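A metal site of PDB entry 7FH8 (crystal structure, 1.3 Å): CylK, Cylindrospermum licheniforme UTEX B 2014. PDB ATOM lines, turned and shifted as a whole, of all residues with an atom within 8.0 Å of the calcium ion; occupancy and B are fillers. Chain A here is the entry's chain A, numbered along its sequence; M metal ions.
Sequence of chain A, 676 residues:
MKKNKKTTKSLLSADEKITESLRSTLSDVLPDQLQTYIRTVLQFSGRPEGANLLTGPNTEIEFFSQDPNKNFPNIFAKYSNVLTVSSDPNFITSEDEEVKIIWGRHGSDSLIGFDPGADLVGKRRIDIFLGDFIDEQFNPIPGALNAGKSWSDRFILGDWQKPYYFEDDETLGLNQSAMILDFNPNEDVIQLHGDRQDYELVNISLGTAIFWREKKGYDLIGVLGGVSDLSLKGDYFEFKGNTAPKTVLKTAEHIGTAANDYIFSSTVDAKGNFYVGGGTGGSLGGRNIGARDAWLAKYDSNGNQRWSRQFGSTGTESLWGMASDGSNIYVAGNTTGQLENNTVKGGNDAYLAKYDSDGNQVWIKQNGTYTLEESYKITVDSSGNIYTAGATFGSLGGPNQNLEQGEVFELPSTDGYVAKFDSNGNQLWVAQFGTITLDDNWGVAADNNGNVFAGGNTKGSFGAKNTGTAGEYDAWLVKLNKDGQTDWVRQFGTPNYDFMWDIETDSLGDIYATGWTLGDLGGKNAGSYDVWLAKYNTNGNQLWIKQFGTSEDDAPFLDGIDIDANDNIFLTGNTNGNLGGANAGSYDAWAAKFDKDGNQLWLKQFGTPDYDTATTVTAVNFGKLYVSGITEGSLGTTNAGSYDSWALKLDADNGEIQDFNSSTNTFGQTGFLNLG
Within 4 Å of the calcium ion: Gly 527, Tyr 529, Asp 530, Thr 550, Glu 552 and Asp 554.
Along chain A the residues within 4 Å of the calcium ion span positions 527 to 554.
The nearest printed residue that does not touch the calcium ion is Ser 551 (4.2 Å).
The calcium ion is bound by the backbone carbonyl oxygen of Glu 552 (2.3 Å), the backbone carbonyl oxygen of Gly 527 (2.3 Å), the backbone carbonyl oxygen of Thr 550 (2.3 Å), the side-chain carboxylate of Asp 530 (2.3 Å), the backbone carbonyl oxygen of Tyr 529 (2.3 Å) and the side-chain carboxylate of Asp 554 (2.4 Å).
The side-chain hydroxyl of Thr 550 sits at hydrogen-bond distance from the backbone NH of Glu 552 (3.0 Å).
The side-chain carboxylate (OE2) of Glu 552 sits at hydrogen-bond distance from the side-chain hydroxyl (OG) of Ser 551 (2.7 Å).
The side-chain amide oxygen of Asn 525 lies within hydrogen-bond range of the backbone NH of Gly 527, at 2.7 Å.
The backbone NH of Ala 526 lies within hydrogen-bond range of the side-chain carboxylate of Asp 530.
The backbone NH of Thr 517 lies within hydrogen-bond range of the backbone carbonyl oxygen of Asp 530, 2.9 Å away.
OD2 of Asp 530 sits at hydrogen-bond distance from NE2 of Gln 547 (3.1 Å).
OD1 of Asp 554 lies within hydrogen-bond range of OG1 of Thr 575, at 2.8 Å.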
ATOM      1  N   THR A 517     -13.209  -9.207   5.813  1.00  0.00           N
ATOM      2  CA  THR A 517     -12.441  -7.978   5.665  1.00  0.00           C
ATOM      3  C   THR A 517     -11.708  -8.008   4.336  1.00  0.00           C
ATOM      4  O   THR A 517     -11.287  -9.061   3.873  1.00  0.00           O
ATOM      5  CB  THR A 517     -11.441  -7.789   6.824  1.00  0.00           C
ATOM      6  OG1 THR A 517     -10.742  -6.550   6.645  1.00  0.00           O
ATOM      7  CG2 THR A 517     -10.422  -8.926   6.874  1.00  0.00           C
ATOM      8  N   LEU A 518     -11.565  -6.825   3.742  1.00  0.00           N
ATOM      9  CA  LEU A 518     -10.681  -6.644   2.595  1.00  0.00           C
ATOM     10  C   LEU A 518      -9.295  -6.161   3.010  1.00  0.00           C
ATOM     11  O   LEU A 518      -8.425  -6.016   2.145  1.00  0.00           O
ATOM     12  CB  LEU A 518     -11.291  -5.674   1.568  1.00  0.00           C
ATOM     13  CG  LEU A 518     -12.538  -6.211   0.853  1.00  0.00           C
ATOM     14  CD1 LEU A 518     -13.253  -5.088   0.087  1.00  0.00           C
ATOM     15  CD2 LEU A 518     -12.178  -7.365  -0.088  1.00  0.00           C
ATOM     16  N   ASN A 525      -3.766 -10.040   4.996  1.00  0.00           N
ATOM     17  CA  ASN A 525      -4.828 -10.553   4.131  1.00  0.00           C
ATOM     18  C   ASN A 525      -4.230 -11.482   3.071  1.00  0.00           C
ATOM     19  O   ASN A 525      -3.259 -11.122   2.397  1.00  0.00           O
ATOM     20  CB  ASN A 525      -5.571  -9.383   3.499  1.00  0.00           C
ATOM     21  CG  ASN A 525      -6.857  -9.818   2.804  1.00  0.00           C
ATOM     22  OD1 ASN A 525      -6.796 -10.542   1.823  1.00  0.00           O
ATOM     23  ND2 ASN A 525      -8.016  -9.386   3.313  1.00  0.00           N
ATOM     24  N   ALA A 526      -4.812 -12.679   2.938  1.00  0.00           N
ATOM     25  CA  ALA A 526      -4.313 -13.677   1.989  1.00  0.00           C
ATOM     26  C   ALA A 526      -4.705 -13.353   0.564  1.00  0.00           C
ATOM     27  O   ALA A 526      -4.117 -13.926  -0.374  1.00  0.00           O
ATOM     28  CB  ALA A 526      -4.826 -15.066   2.379  1.00  0.00           C
ATOM     29  N   GLY A 527      -5.673 -12.468   0.385  1.00  0.00           N
ATOM     30  CA  GLY A 527      -6.172 -12.081  -0.919  1.00  0.00           C
ATOM     31  C   GLY A 527      -7.667 -11.885  -0.871  1.00  0.00           C
ATOM     32  O   GLY A 527      -8.388 -12.646  -0.195  1.00  0.00           O
ATOM     33  N   SER A 528      -8.163 -10.855  -1.560  1.00  0.00           N
ATOM     34  CA  SER A 528      -9.610 -10.657  -1.722  1.00  0.00           C
ATOM     35  C   SER A 528     -10.265 -10.551  -0.336  1.00  0.00           C
ATOM     36  O   SER A 528      -9.696  -9.964   0.591  1.00  0.00           O
ATOM     37  CB  SER A 528     -10.126 -11.771  -2.634  1.00  0.00           C
ATOM     38  OG  SER A 528     -11.524 -11.673  -2.867  1.00  0.00           O
ATOM     39  N   TYR A 529     -11.458 -11.118  -0.172  1.00  0.00           N
ATOM     40  CA  TYR A 529     -12.131 -11.188   1.116  1.00  0.00           C
ATOM     41  C   TYR A 529     -11.508 -12.295   1.949  1.00  0.00           C
ATOM     42  O   TYR A 529     -11.222 -13.373   1.424  1.00  0.00           O
ATOM     43  CB  TYR A 529     -13.609 -11.545   0.899  1.00  0.00           C
ATOM     44  CG  TYR A 529     -14.401 -10.487   0.169  1.00  0.00           C
ATOM     45  CD1 TYR A 529     -14.402 -10.419  -1.231  1.00  0.00           C
ATOM     46  CD2 TYR A 529     -15.144  -9.540   0.860  1.00  0.00           C
ATOM     47  CE1 TYR A 529     -15.117  -9.446  -1.902  1.00  0.00           C
ATOM     48  CE2 TYR A 529     -15.878  -8.562   0.204  1.00  0.00           C
ATOM     49  CZ  TYR A 529     -15.855  -8.517  -1.185  1.00  0.00           C
ATOM     50  OH  TYR A 529     -16.565  -7.550  -1.861  1.00  0.00           O
ATOM     51  N   ASP A 530     -11.286 -12.017   3.242  1.00  0.00           N
ATOM     52  CA  ASP A 530     -10.882 -13.026   4.223  1.00  0.00           C
ATOM     53  C   ASP A 530     -11.895 -13.026   5.362  1.00  0.00           C
ATOM     54  O   ASP A 530     -12.589 -12.039   5.617  1.00  0.00           O
ATOM     55  CB  ASP A 530      -9.520 -12.720   4.853  1.00  0.00           C
ATOM     56  CG  ASP A 530      -8.320 -13.182   4.022  1.00  0.00           C
ATOM     57  OD1 ASP A 530      -8.474 -13.792   2.942  1.00  0.00           O
ATOM     58  OD2 ASP A 530      -7.189 -12.910   4.509  1.00  0.00           O
ATOM     59  N   VAL A 531     -11.931 -14.145   6.106  1.00  0.00           N
ATOM     60  CA  VAL A 531     -12.803 -14.313   7.265  1.00  0.00           C
ATOM     61  C   VAL A 531     -12.113 -13.777   8.512  1.00  0.00           C
ATOM     62  O   VAL A 531     -10.895 -13.946   8.687  1.00  0.00           O
ATOM     63  CB  VAL A 531     -13.155 -15.805   7.466  1.00  0.00           C
ATOM     64  CG1 VAL A 531     -14.099 -15.978   8.662  1.00  0.00           C
ATOM     65  CG2 VAL A 531     -13.782 -16.400   6.217  1.00  0.00           C
ATOM     66  N   GLN A 547      -7.860 -14.004  11.752  1.00  0.00           N
ATOM     67  CA  GLN A 547      -8.188 -13.810  10.342  1.00  0.00           C
ATOM     68  C   GLN A 547      -7.626 -14.977   9.564  1.00  0.00           C
ATOM     69  O   GLN A 547      -6.502 -15.415   9.816  1.00  0.00           O
ATOM     70  CB  GLN A 547      -7.603 -12.493   9.815  1.00  0.00           C
ATOM     71  CG  GLN A 547      -7.913 -12.222   8.342  1.00  0.00           C
ATOM     72  CD  GLN A 547      -7.574 -10.797   7.912  1.00  0.00           C
ATOM     73  OE1 GLN A 547      -7.618  -9.870   8.727  1.00  0.00           O
ATOM     74  NE2 GLN A 547      -7.295 -10.601   6.615  1.00  0.00           N
ATOM     75  N   PHE A 548      -8.414 -15.493   8.622  1.00  0.00           N
ATOM     76  CA  PHE A 548      -7.966 -16.637   7.830  1.00  0.00           C
ATOM     77  C   PHE A 548      -8.660 -16.646   6.482  1.00  0.00           C
ATOM     78  O   PHE A 548      -9.697 -16.012   6.290  1.00  0.00           O
ATOM     79  CB  PHE A 548      -8.180 -17.976   8.557  1.00  0.00           C
ATOM     80  CG  PHE A 548      -9.630 -18.368   8.727  1.00  0.00           C
ATOM     81  CD1 PHE A 548     -10.384 -17.864   9.776  1.00  0.00           C
ATOM     82  CD2 PHE A 548     -10.242 -19.226   7.815  1.00  0.00           C
ATOM     83  CE1 PHE A 548     -11.704 -18.227   9.942  1.00  0.00           C
ATOM     84  CE2 PHE A 548     -11.578 -19.587   7.965  1.00  0.00           C
ATOM     85  CZ  PHE A 548     -12.307 -19.083   9.034  1.00  0.00           C
ATOM     86  N   GLY A 549      -8.081 -17.382   5.542  1.00  0.00           N
ATOM     87  CA  GLY A 549      -8.698 -17.492   4.238  1.00  0.00           C
ATOM     88  C   GLY A 549      -7.735 -18.087   3.238  1.00  0.00           C
ATOM     89  O   GLY A 549      -6.706 -18.667   3.589  1.00  0.00           O
ATOM     90  N   THR A 550      -8.113 -17.939   1.969  1.00  0.00           N
ATOM     91  CA  THR A 550      -7.316 -18.293   0.806  1.00  0.00           C
ATOM     92  C   THR A 550      -7.008 -17.018   0.037  1.00  0.00           C
ATOM     93  O   THR A 550      -7.476 -15.925   0.377  1.00  0.00           O
ATOM     94  CB  THR A 550      -8.083 -19.249  -0.129  1.00  0.00           C
ATOM     95  OG1 THR A 550      -9.170 -18.544  -0.733  1.00  0.00           O
ATOM     96  CG2 THR A 550      -8.595 -20.483   0.586  1.00  0.00           C
ATOM     97  N   SER A 551      -6.232 -17.175  -1.030  1.00  0.00           N
ATOM     98  CA  SER A 551      -5.993 -16.075  -1.961  1.00  0.00           C
ATOM     99  C   SER A 551      -7.273 -15.591  -2.626  1.00  0.00           C
ATOM    100  O   SER A 551      -7.280 -14.490  -3.187  1.00  0.00           O
ATOM    101  CB  SER A 551      -4.966 -16.500  -3.011  1.00  0.00           C
ATOM    102  OG  SER A 551      -5.457 -17.597  -3.764  1.00  0.00           O
ATOM    103  N   GLU A 552      -8.350 -16.378  -2.577  1.00  0.00           N
ATOM    104  CA  GLU A 552      -9.598 -16.054  -3.234  1.00  0.00           C
ATOM    105  C   GLU A 552     -10.578 -15.447  -2.227  1.00  0.00           C
ATOM    106  O   GLU A 552     -10.178 -14.943  -1.173  1.00  0.00           O
ATOM    107  CB  GLU A 552     -10.149 -17.300  -3.958  1.00  0.00           C
ATOM    108  CG  GLU A 552      -9.094 -18.021  -4.782  1.00  0.00           C
ATOM    109  CD  GLU A 552      -8.401 -17.097  -5.753  1.00  0.00           C
ATOM    110  OE1 GLU A 552      -9.108 -16.426  -6.525  1.00  0.00           O
ATOM    111  OE2 GLU A 552      -7.146 -17.021  -5.743  1.00  0.00           O
ATOM    112  N   ASP A 553     -11.869 -15.489  -2.557  1.00  0.00           N
ATOM    113  CA  ASP A 553     -12.898 -14.772  -1.814  1.00  0.00           C
ATOM    114  C   ASP A 553     -13.480 -15.710  -0.754  1.00  0.00           C
ATOM    115  O   ASP A 553     -14.127 -16.707  -1.097  1.00  0.00           O
ATOM    116  CB  ASP A 553     -13.938 -14.328  -2.859  1.00  0.00           C
ATOM    117  CG  ASP A 553     -15.126 -13.601  -2.273  1.00  0.00           C
ATOM    118  OD1 ASP A 553     -15.370 -13.637  -1.056  1.00  0.00           O
ATOM    119  OD2 ASP A 553     -15.861 -13.016  -3.104  1.00  0.00           O
ATOM    120  N   ASP A 554     -13.258 -15.381   0.531  1.00  0.00           N
ATOM    121  CA  ASP A 554     -13.715 -16.211   1.647  1.00  0.00           C
ATOM    122  C   ASP A 554     -14.496 -15.322   2.609  1.00  0.00           C
ATOM    123  O   ASP A 554     -13.988 -14.265   2.998  1.00  0.00           O
ATOM    124  CB  ASP A 554     -12.500 -16.710   2.438  1.00  0.00           C
ATOM    125  CG  ASP A 554     -11.391 -17.165   1.527  1.00  0.00           C
ATOM    126  OD1 ASP A 554     -11.459 -18.207   0.833  1.00  0.00           O
ATOM    127  OD2 ASP A 554     -10.379 -16.448   1.566  1.00  0.00           O
ATOM    128  N   ALA A 555     -15.691 -15.764   3.027  1.00  0.00           N
ATOM    129  CA  ALA A 555     -16.482 -14.940   3.954  1.00  0.00           C
ATOM    130  C   ALA A 555     -17.474 -15.805   4.719  1.00  0.00           C
ATOM    131  O   ALA A 555     -17.979 -16.787   4.152  1.00  0.00           O
ATOM    132  CB  ALA A 555     -17.236 -13.847   3.194  1.00  0.00           C
ATOM    133  N   THR A 575     -17.023 -19.616  -0.062  1.00  0.00           N
ATOM    134  CA  THR A 575     -15.695 -19.346  -0.589  1.00  0.00           C
ATOM    135  C   THR A 575     -15.659 -19.731  -2.058  1.00  0.00           C
ATOM    136  O   THR A 575     -16.274 -20.726  -2.450  1.00  0.00           O
ATOM    137  CB  THR A 575     -14.615 -20.134   0.184  1.00  0.00           C
ATOM    138  OG1 THR A 575     -13.328 -19.879  -0.392  1.00  0.00           O
ATOM    139  CG2 THR A 575     -14.865 -21.631   0.136  1.00  0.00           C
ATOM    140  N   ASN A 576     -14.925 -18.975  -2.861  1.00  0.00           N
ATOM    141  CA  ASN A 576     -14.623 -19.438  -4.217  1.00  0.00           C
ATOM    142  C   ASN A 576     -13.176 -19.890  -4.346  1.00  0.00           C
ATOM    143  O   ASN A 576     -12.669 -20.027  -5.458  1.00  0.00           O
ATOM    144  CB  ASN A 576     -15.059 -18.447  -5.290  1.00  0.00           C
ATOM    145  CG  ASN A 576     -14.245 -17.175  -5.293  1.00  0.00           C
ATOM    146  OD1 ASN A 576     -13.320 -17.015  -4.478  1.00  0.00           O
ATOM    147  ND2 ASN A 576     -14.579 -16.256  -6.194  1.00  0.00           N
ATOM    148  N   GLY A 577     -12.519 -20.164  -3.213  1.00  0.00           N
ATOM    149  CA  GLY A 577     -11.206 -20.755  -3.207  1.00  0.00           C
ATOM    150  C   GLY A 577     -11.212 -22.179  -2.687  1.00  0.00           C
ATOM    151  O   GLY A 577     -12.270 -22.810  -2.530  1.00  0.00           O
ATOM    152  N   LEU A 579     -10.620 -23.545   0.341  1.00  0.00           N
ATOM    153  CA  LEU A 579     -10.460 -23.200   1.753  1.00  0.00           C
ATOM    154  C   LEU A 579     -10.394 -24.448   2.630  1.00  0.00           C
ATOM    155  O   LEU A 579      -9.419 -24.635   3.378  1.00  0.00           O
ATOM    156  CB  LEU A 579     -11.592 -22.273   2.190  1.00  0.00           C
ATOM    157  CG  LEU A 579     -11.582 -21.784   3.641  1.00  0.00           C
ATOM    158  CD1 LEU A 579     -10.301 -20.981   3.934  1.00  0.00           C
ATOM    159  CD2 LEU A 579     -12.835 -20.933   3.916  1.00  0.00           C
HETATM  160 CA    CA M   1      -9.250 -14.505   0.866  1.00  0.00          CA
